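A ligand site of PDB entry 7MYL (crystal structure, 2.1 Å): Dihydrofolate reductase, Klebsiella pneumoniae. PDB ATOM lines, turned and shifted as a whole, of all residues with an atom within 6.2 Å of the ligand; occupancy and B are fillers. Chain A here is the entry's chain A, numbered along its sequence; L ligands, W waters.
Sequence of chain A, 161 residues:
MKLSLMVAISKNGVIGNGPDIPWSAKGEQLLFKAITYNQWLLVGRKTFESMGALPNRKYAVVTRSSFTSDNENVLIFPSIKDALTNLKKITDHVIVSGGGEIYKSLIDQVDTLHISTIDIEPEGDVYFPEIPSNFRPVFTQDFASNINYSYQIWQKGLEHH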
ATOM      1  N   MET A   6      -7.520 -11.971   3.284  1.00  0.00           N
ATOM      2  CA  MET A   6      -8.675 -12.875   3.399  1.00  0.00           C
ATOM      3  C   MET A   6      -8.950 -13.492   2.032  1.00  0.00           C
ATOM      4  O   MET A   6      -8.993 -12.715   1.034  1.00  0.00           O
ATOM      5  CB  MET A   6      -9.902 -12.123   3.918  1.00  0.00           C
ATOM      6  CG  MET A   6     -11.031 -13.043   4.243  1.00  0.00           C
ATOM      7  SD  MET A   6     -12.010 -12.429   5.596  1.00  0.00           S
ATOM      8  CE  MET A   6     -12.989 -13.887   5.936  1.00  0.00           C
ATOM      9  N   VAL A   7      -9.125 -14.821   2.005  1.00  0.00           N
ATOM     10  CA  VAL A   7      -9.380 -15.633   0.781  1.00  0.00           C
ATOM     11  C   VAL A   7     -10.188 -16.892   1.123  1.00  0.00           C
ATOM     12  O   VAL A   7     -10.057 -17.419   2.255  1.00  0.00           O
ATOM     13  CB  VAL A   7      -8.068 -16.048   0.089  1.00  0.00           C
ATOM     14  CG1 VAL A   7      -7.280 -17.014   0.956  1.00  0.00           C
ATOM     15  CG2 VAL A   7      -8.317 -16.646  -1.281  1.00  0.00           C
ATOM     16  N   ALA A   8     -10.942 -17.379   0.138  1.00  0.00           N
ATOM     17  CA  ALA A   8     -11.596 -18.695   0.093  1.00  0.00           C
ATOM     18  C   ALA A   8     -10.925 -19.530  -1.010  1.00  0.00           C
ATOM     19  O   ALA A   8     -10.863 -19.041  -2.143  1.00  0.00           O
ATOM     20  CB  ALA A   8     -13.070 -18.536  -0.146  1.00  0.00           C
ATOM     21  N   GLY A  16     -11.601 -19.387  -4.738  1.00  0.00           N
ATOM     22  CA  GLY A  16     -13.049 -19.609  -4.795  1.00  0.00           C
ATOM     23  C   GLY A  16     -13.813 -18.374  -4.364  1.00  0.00           C
ATOM     24  O   GLY A  16     -14.982 -18.513  -4.008  1.00  0.00           O
ATOM     25  N   ASN A  17     -13.156 -17.210  -4.385  1.00  0.00           N
ATOM     26  CA  ASN A  17     -13.780 -15.897  -4.059  1.00  0.00           C
ATOM     27  C   ASN A  17     -14.915 -15.613  -5.058  1.00  0.00           C
ATOM     28  O   ASN A  17     -15.955 -15.129  -4.599  1.00  0.00           O
ATOM     29  CB  ASN A  17     -12.795 -14.730  -4.150  1.00  0.00           C
ATOM     30  CG  ASN A  17     -11.723 -14.742  -3.084  1.00  0.00           C
ATOM     31  OD1 ASN A  17     -10.805 -13.908  -3.092  1.00  0.00           O
ATOM     32  ND2 ASN A  17     -11.822 -15.688  -2.178  1.00  0.00           N
ATOM     33  N   GLY A  18     -14.670 -15.889  -6.350  1.00  0.00           N
ATOM     34  CA  GLY A  18     -15.378 -15.355  -7.541  1.00  0.00           C
ATOM     35  C   GLY A  18     -16.891 -15.533  -7.478  1.00  0.00           C
ATOM     36  O   GLY A  18     -17.391 -16.356  -6.692  1.00  0.00           O
ATOM     37  N   PRO A  19     -17.668 -14.800  -8.320  1.00  0.00           N
ATOM     38  CA  PRO A  19     -19.124 -14.699  -8.172  1.00  0.00           C
ATOM     39  C   PRO A  19     -19.930 -15.952  -8.529  1.00  0.00           C
ATOM     40  O   PRO A  19     -20.821 -16.326  -7.783  1.00  0.00           O
ATOM     41  CB  PRO A  19     -19.489 -13.539  -9.115  1.00  0.00           C
ATOM     42  CG  PRO A  19     -18.408 -13.542 -10.179  1.00  0.00           C
ATOM     43  CD  PRO A  19     -17.157 -14.023  -9.466  1.00  0.00           C
ATOM     44  N   ASP A  20     -19.607 -16.575  -9.666  1.00  0.00           N
ATOM     45  CA  ASP A  20     -20.367 -17.735 -10.214  1.00  0.00           C
ATOM     46  C   ASP A  20     -19.490 -18.985 -10.091  1.00  0.00           C
ATOM     47  O   ASP A  20     -19.513 -19.821 -11.017  1.00  0.00           O
ATOM     48  CB  ASP A  20     -20.853 -17.440 -11.639  1.00  0.00           C
ATOM     49  CG  ASP A  20     -21.795 -16.241 -11.739  1.00  0.00           C
ATOM     50  OD1 ASP A  20     -22.279 -15.780 -10.682  1.00  0.00           O
ATOM     51  OD2 ASP A  20     -22.046 -15.781 -12.869  1.00  0.00           O
ATOM     52  N   GLU A  28     -20.112 -19.943   4.453  1.00  0.00           N
ATOM     53  CA  GLU A  28     -18.695 -19.486   4.443  1.00  0.00           C
ATOM     54  C   GLU A  28     -18.618 -17.961   4.249  1.00  0.00           C
ATOM     55  O   GLU A  28     -17.811 -17.318   4.940  1.00  0.00           O
ATOM     56  CB  GLU A  28     -17.882 -20.242   3.389  1.00  0.00           C
ATOM     57  CG  GLU A  28     -16.412 -19.875   3.381  1.00  0.00           C
ATOM     58  CD  GLU A  28     -16.045 -18.657   2.563  1.00  0.00           C
ATOM     59  OE1 GLU A  28     -16.690 -18.433   1.517  1.00  0.00           O
ATOM     60  OE2 GLU A  28     -15.117 -17.931   2.966  1.00  0.00           O
ATOM     61  N   GLN A  29     -19.451 -17.395   3.362  1.00  0.00           N
ATOM     62  CA  GLN A  29     -19.357 -15.947   2.999  1.00  0.00           C
ATOM     63  C   GLN A  29     -19.745 -15.081   4.217  1.00  0.00           C
ATOM     64  O   GLN A  29     -19.444 -13.862   4.203  1.00  0.00           O
ATOM     65  CB  GLN A  29     -20.123 -15.691   1.690  1.00  0.00           C
ATOM     66  CG  GLN A  29     -21.338 -14.770   1.786  1.00  0.00           C
ATOM     67  CD  GLN A  29     -21.486 -13.871   0.586  1.00  0.00           C
ATOM     68  OE1 GLN A  29     -20.723 -13.934  -0.385  1.00  0.00           O
ATOM     69  NE2 GLN A  29     -22.476 -12.991   0.629  1.00  0.00           N
ATOM     70  N   LEU A  31     -18.237 -15.303   7.060  1.00  0.00           N
ATOM     71  CA  LEU A  31     -16.920 -14.986   7.683  1.00  0.00           C
ATOM     72  C   LEU A  31     -16.378 -13.705   7.040  1.00  0.00           C
ATOM     73  O   LEU A  31     -15.883 -12.820   7.787  1.00  0.00           O
ATOM     74  CB  LEU A  31     -15.956 -16.162   7.493  1.00  0.00           C
ATOM     75  CG  LEU A  31     -16.315 -17.428   8.255  1.00  0.00           C
ATOM     76  CD1 LEU A  31     -15.576 -18.642   7.702  1.00  0.00           C
ATOM     77  CD2 LEU A  31     -16.018 -17.270   9.727  1.00  0.00           C
ATOM     78  N   PHE A  32     -16.439 -13.655   5.706  1.00  0.00           N
ATOM     79  CA  PHE A  32     -15.912 -12.530   4.892  1.00  0.00           C
ATOM     80  C   PHE A  32     -16.691 -11.272   5.269  1.00  0.00           C
ATOM     81  O   PHE A  32     -16.064 -10.225   5.492  1.00  0.00           O
ATOM     82  CB  PHE A  32     -16.024 -12.835   3.398  1.00  0.00           C
ATOM     83  CG  PHE A  32     -15.582 -11.690   2.534  1.00  0.00           C
ATOM     84  CD1 PHE A  32     -14.240 -11.383   2.414  1.00  0.00           C
ATOM     85  CD2 PHE A  32     -16.517 -10.864   1.908  1.00  0.00           C
ATOM     86  CE1 PHE A  32     -13.828 -10.327   1.626  1.00  0.00           C
ATOM     87  CE2 PHE A  32     -16.100  -9.795   1.120  1.00  0.00           C
ATOM     88  CZ  PHE A  32     -14.761  -9.525   0.993  1.00  0.00           C
ATOM     89  N   LYS A  46     -10.625  -6.706 -11.343  1.00  0.00           N
ATOM     90  CA  LYS A  46     -11.589  -7.809 -11.624  1.00  0.00           C
ATOM     91  C   LYS A  46     -12.365  -8.137 -10.344  1.00  0.00           C
ATOM     92  O   LYS A  46     -13.600  -8.343 -10.433  1.00  0.00           O
ATOM     93  CB  LYS A  46     -10.911  -9.084 -12.119  1.00  0.00           C
ATOM     94  CG  LYS A  46      -9.940  -8.903 -13.286  1.00  0.00           C
ATOM     95  CD  LYS A  46      -8.748  -9.850 -13.214  1.00  0.00           C
ATOM     96  CE  LYS A  46      -7.552  -9.433 -14.055  1.00  0.00           C
ATOM     97  NZ  LYS A  46      -7.884  -9.365 -15.506  1.00  0.00           N
ATOM     98  N   THR A  47     -11.661  -8.197  -9.196  1.00  0.00           N
ATOM     99  CA  THR A  47     -12.272  -8.470  -7.865  1.00  0.00           C
ATOM    100  C   THR A  47     -13.278  -7.365  -7.563  1.00  0.00           C
ATOM    101  O   THR A  47     -14.446  -7.692  -7.246  1.00  0.00           O
ATOM    102  CB  THR A  47     -11.210  -8.654  -6.768  1.00  0.00           C
ATOM    103  OG1 THR A  47     -10.402  -9.763  -7.131  1.00  0.00           O
ATOM    104  CG2 THR A  47     -11.782  -8.898  -5.391  1.00  0.00           C
ATOM    105  N   PHE A  48     -12.901  -6.094  -7.727  1.00  0.00           N
ATOM    106  CA  PHE A  48     -13.818  -4.963  -7.413  1.00  0.00           C
ATOM    107  C   PHE A  48     -15.098  -5.144  -8.224  1.00  0.00           C
ATOM    108  O   PHE A  48     -16.164  -5.224  -7.614  1.00  0.00           O
ATOM    109  CB  PHE A  48     -13.199  -3.581  -7.622  1.00  0.00           C
ATOM    110  CG  PHE A  48     -14.172  -2.482  -7.272  1.00  0.00           C
ATOM    111  CD1 PHE A  48     -14.477  -2.198  -5.951  1.00  0.00           C
ATOM    112  CD2 PHE A  48     -14.841  -1.795  -8.259  1.00  0.00           C
ATOM    113  CE1 PHE A  48     -15.397  -1.210  -5.630  1.00  0.00           C
ATOM    114  CE2 PHE A  48     -15.778  -0.815  -7.944  1.00  0.00           C
ATOM    115  CZ  PHE A  48     -16.055  -0.535  -6.633  1.00  0.00           C
ATOM    116  N   SER A  50     -16.485  -7.738  -9.971  1.00  0.00           N
ATOM    117  CA  SER A  50     -17.270  -8.960  -9.646  1.00  0.00           C
ATOM    118  C   SER A  50     -18.052  -8.748  -8.332  1.00  0.00           C
ATOM    119  O   SER A  50     -19.239  -9.106  -8.281  1.00  0.00           O
ATOM    120  CB  SER A  50     -16.401 -10.214  -9.560  1.00  0.00           C
ATOM    121  OG  SER A  50     -15.608 -10.374 -10.713  1.00  0.00           O
ATOM    122  N   MET A  51     -17.389  -8.173  -7.308  1.00  0.00           N
ATOM    123  CA  MET A  51     -17.931  -7.988  -5.943  1.00  0.00           C
ATOM    124  C   MET A  51     -18.937  -6.836  -5.899  1.00  0.00           C
ATOM    125  O   MET A  51     -19.956  -6.961  -5.197  1.00  0.00           O
ATOM    126  CB  MET A  51     -16.782  -7.685  -4.963  1.00  0.00           C
ATOM    127  CG  MET A  51     -17.172  -7.768  -3.498  1.00  0.00           C
ATOM    128  SD  MET A  51     -15.881  -7.199  -2.362  1.00  0.00           S
ATOM    129  CE  MET A  51     -14.399  -7.963  -3.023  1.00  0.00           C
ATOM    130  N   GLY A  52     -18.651  -5.741  -6.615  1.00  0.00           N
ATOM    131  CA  GLY A  52     -19.370  -4.447  -6.457  1.00  0.00           C
ATOM    132  C   GLY A  52     -18.997  -3.767  -5.155  1.00  0.00           C
ATOM    133  O   GLY A  52     -18.301  -4.392  -4.329  1.00  0.00           O
ATOM    134  N   LEU A  54     -19.917  -3.082  -1.906  1.00  0.00           N
ATOM    135  CA  LEU A  54     -20.891  -3.666  -0.937  1.00  0.00           C
ATOM    136  C   LEU A  54     -21.074  -2.688   0.210  1.00  0.00           C
ATOM    137  O   LEU A  54     -20.168  -1.975   0.596  1.00  0.00           O
ATOM    138  CB  LEU A  54     -20.398  -5.029  -0.437  1.00  0.00           C
ATOM    139  CG  LEU A  54     -20.381  -6.166  -1.458  1.00  0.00           C
ATOM    140  CD1 LEU A  54     -19.972  -7.485  -0.813  1.00  0.00           C
ATOM    141  CD2 LEU A  54     -21.739  -6.328  -2.141  1.00  0.00           C
ATOM    142  N   ARG A  57     -18.266  -1.337   3.326  1.00  0.00           N
ATOM    143  CA  ARG A  57     -16.870  -1.635   2.927  1.00  0.00           C
ATOM    144  C   ARG A  57     -16.290  -0.434   2.190  1.00  0.00           C
ATOM    145  O   ARG A  57     -17.044   0.262   1.494  1.00  0.00           O
ATOM    146  CB  ARG A  57     -16.828  -2.909   2.087  1.00  0.00           C
ATOM    147  CG  ARG A  57     -16.716  -4.186   2.918  1.00  0.00           C
ATOM    148  CD  ARG A  57     -18.005  -4.607   3.601  1.00  0.00           C
ATOM    149  NE  ARG A  57     -18.135  -6.047   3.400  1.00  0.00           N
ATOM    150  CZ  ARG A  57     -19.189  -6.691   2.911  1.00  0.00           C
ATOM    151  NH1 ARG A  57     -20.314  -6.052   2.612  1.00  0.00           N
ATOM    152  NH2 ARG A  57     -19.127  -8.001   2.751  1.00  0.00           N
ATOM    153  N   VAL A  96      -6.312  -7.327   2.394  1.00  0.00           N
ATOM    154  CA  VAL A  96      -6.081  -7.754   0.985  1.00  0.00           C
ATOM    155  C   VAL A  96      -7.117  -8.827   0.670  1.00  0.00           C
ATOM    156  O   VAL A  96      -7.099  -9.857   1.330  1.00  0.00           O
ATOM    157  CB  VAL A  96      -4.650  -8.270   0.816  1.00  0.00           C
ATOM    158  CG1 VAL A  96      -4.378  -8.689  -0.620  1.00  0.00           C
ATOM    159  CG2 VAL A  96      -3.620  -7.252   1.290  1.00  0.00           C
ATOM    160  N   SER A  97      -8.028  -8.571  -0.263  1.00  0.00           N
ATOM    161  CA  SER A  97      -9.269  -9.356  -0.463  1.00  0.00           C
ATOM    162  C   SER A  97      -9.358  -9.892  -1.905  1.00  0.00           C
ATOM    163  O   SER A  97     -10.441 -10.406  -2.293  1.00  0.00           O
ATOM    164  CB  SER A  97     -10.446  -8.521  -0.065  1.00  0.00           C
ATOM    165  OG  SER A  97     -10.237  -8.051   1.261  1.00  0.00           O
ATOM    166  N   GLY A  98      -8.263  -9.773  -2.650  1.00  0.00           N
ATOM    167  CA  GLY A  98      -7.935 -10.703  -3.744  1.00  0.00           C
ATOM    168  C   GLY A  98      -7.763 -10.075  -5.111  1.00  0.00           C
ATOM    169  O   GLY A  98      -7.776  -8.828  -5.230  1.00  0.00           O
ATOM    170  N   TYR A 103      -2.650 -11.196  -4.279  1.00  0.00           N
ATOM    171  CA  TYR A 103      -2.246 -12.102  -3.167  1.00  0.00           C
ATOM    172  C   TYR A 103      -0.762 -12.482  -3.277  1.00  0.00           C
ATOM    173  O   TYR A 103      -0.044 -12.399  -2.263  1.00  0.00           O
ATOM    174  CB  TYR A 103      -3.073 -13.389  -3.157  1.00  0.00           C
ATOM    175  CG  TYR A 103      -4.531 -13.250  -2.763  1.00  0.00           C
ATOM    176  CD1 TYR A 103      -4.909 -12.559  -1.626  1.00  0.00           C
ATOM    177  CD2 TYR A 103      -5.510 -13.884  -3.507  1.00  0.00           C
ATOM    178  CE1 TYR A 103      -6.245 -12.489  -1.248  1.00  0.00           C
ATOM    179  CE2 TYR A 103      -6.835 -13.833  -3.133  1.00  0.00           C
ATOM    180  CZ  TYR A 103      -7.209 -13.130  -1.996  1.00  0.00           C
ATOM    181  OH  TYR A 103      -8.525 -13.058  -1.675  1.00  0.00           O
ATOM    182  N   HIS A 114      -6.644 -14.832   6.871  1.00  0.00           N
ATOM    183  CA  HIS A 114      -7.964 -15.455   7.097  1.00  0.00           C
ATOM    184  C   HIS A 114      -8.289 -16.385   5.937  1.00  0.00           C
ATOM    185  O   HIS A 114      -8.674 -15.875   4.852  1.00  0.00           O
ATOM    186  CB  HIS A 114      -9.048 -14.374   7.228  1.00  0.00           C
ATOM    187  CG  HIS A 114      -8.909 -13.531   8.442  1.00  0.00           C
ATOM    188  ND1 HIS A 114      -9.563 -13.844   9.618  1.00  0.00           N
ATOM    189  CD2 HIS A 114      -8.213 -12.398   8.682  1.00  0.00           C
ATOM    190  CE1 HIS A 114      -9.277 -12.936  10.525  1.00  0.00           C
ATOM    191  NE2 HIS A 114      -8.424 -12.052   9.979  1.00  0.00           N
ATOM    192  N   SER A 116     -10.450 -19.616   4.342  1.00  0.00           N
ATOM    193  CA  SER A 116     -11.579 -20.569   4.256  1.00  0.00           C
ATOM    194  C   SER A 116     -11.176 -21.645   3.247  1.00  0.00           C
ATOM    195  O   SER A 116     -10.943 -21.267   2.081  1.00  0.00           O
ATOM    196  CB  SER A 116     -12.859 -19.889   3.843  1.00  0.00           C
ATOM    197  OG  SER A 116     -13.113 -18.759   4.656  1.00  0.00           O
HETATM  198  C1  LIG L   1     -14.639 -13.635  -0.766  1.00  0.00           C
HETATM  199  N1  LIG L   1     -14.648 -14.594   0.168  1.00  0.00           N
HETATM  200  C2  LIG L   1     -13.573 -14.668   0.982  1.00  0.00           C
HETATM  201  N2  LIG L   1     -13.570 -15.595   1.938  1.00  0.00           N
HETATM  202  N3  LIG L   1     -12.498 -13.863   0.901  1.00  0.00           N
HETATM  203  C3  LIG L   1     -12.495 -12.923  -0.055  1.00  0.00           C
HETATM  204  N4  LIG L   1     -11.413 -12.121  -0.122  1.00  0.00           N
HETATM  205  C4  LIG L   1     -13.581 -12.752  -0.941  1.00  0.00           C
HETATM  206  C5  LIG L   1     -13.588 -11.662  -1.976  1.00  0.00           C
HETATM  207  C6  LIG L   1     -14.829 -11.553  -2.832  1.00  0.00           C
HETATM  208  C7  LIG L   1     -16.091 -11.350  -2.287  1.00  0.00           C
HETATM  209  C8  LIG L   1     -17.218 -11.263  -3.103  1.00  0.00           C
HETATM  210  O1  LIG L   1     -18.512 -11.074  -2.679  1.00  0.00           O
HETATM  211  C9  LIG L   1     -18.730 -10.888  -1.276  1.00  0.00           C
HETATM  212  C10 LIG L   1     -17.085 -11.379  -4.497  1.00  0.00           C
HETATM  213  O2  LIG L   1     -18.189 -11.302  -5.301  1.00  0.00           O
HETATM  214  C11 LIG L   1     -19.049 -12.440  -5.271  1.00  0.00           C
HETATM  215  C12 LIG L   1     -15.820 -11.591  -5.039  1.00  0.00           C
HETATM  216  O3  LIG L   1     -15.759 -11.702  -6.398  1.00  0.00           O
HETATM  217  C13 LIG L   1     -14.468 -11.938  -6.981  1.00  0.00           C
HETATM  218  C14 LIG L   1     -14.706 -11.657  -4.210  1.00  0.00           C
HETATM  219  O   HOH W   1     -16.531 -16.397  -0.024  1.00  0.00           O
HETATM  220  O   HOH W   2     -11.665 -16.379   4.204  1.00  0.00           O
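A nitrogen (N4) of the ligand is in hydrogen-bond range of the backbone carbonyl oxygen (O) of Met 6 (2.7 Å). A nitrogen (N4) of the ligand sits at hydrogen-bond distance from the backbone carbonyl oxygen (O) of Ser 97, 2.9 Å away. OE2 of Glu 28 lies within hydrogen-bond range of N2 of the ligand (3.0 Å). A nitrogen (N4) of the ligand sits at hydrogen-bond distance from the side-chain hydroxyl of Tyr 103, at 3.4 Å.
N of Met 6 lies within hydrogen-bond range of O of Val 96. OH of Tyr 103 sits close to O of Ser 97 (3.3 Å). OG of Ser 116 sits at hydrogen-bond distance from OE2 of Glu 28 (2.7 Å). The side-chain hydroxyl (OH) of Tyr 103 lies within hydrogen-bond range of the side-chain amide oxygen (OD1) of Asn 17 (2.8 Å). The backbone NH of Ala 8 lies close to the side-chain amide nitrogen of Asn 17 (3.0 Å). The side-chain hydroxyl (OG) of Ser 50 sits at hydrogen-bond distance from the backbone carbonyl oxygen (O) of Lys 46. O of Val 7 lies within hydrogen-bond range of N of Ser 116, 3.1 Å away. O of His 114 is in hydrogen-bond range of N of Val 7 (3.1 Å).
Merely in contact with the ligand: Phe 32 (3.4 Å), Met 51 (3.4 Å), Asn 17 (3.5 Å), Ser 50 (3.6 Å), Gly 18 (3.6 Å), Val 7 (3.6 Å), Ala 8 (3.6 Å), Leu 54 (3.7 Å), Pro 19 (3.7 Å) and Gln 29 (3.7 Å). Hydrophobic or aromatic side chains within 4 Å of the ligand: Met 6, Ala 8, Phe 32, Met 51 and Leu 54. 14 residues have an atom within 4 Å of the ligand: Met 6, Val 7, Ala 8, Asn 17, Gly 18, Pro 19, Glu 28, Gln 29, Phe 32, Ser 50, Met 51, Leu 54, Ser 97 and Tyr 103. The nearest printed residue that does not touch the ligand is Thr 47 (4.2 Å).
Water W1 bridges OE1 of Glu 28 and N1 of the ligand. Water W2 lies within hydrogen-bond range of O of Val 7 (2.7 Å), OG of Ser 116 (2.8 Å), N2 of the ligand (3.1 Å) and O of His 114 (3.1 Å).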
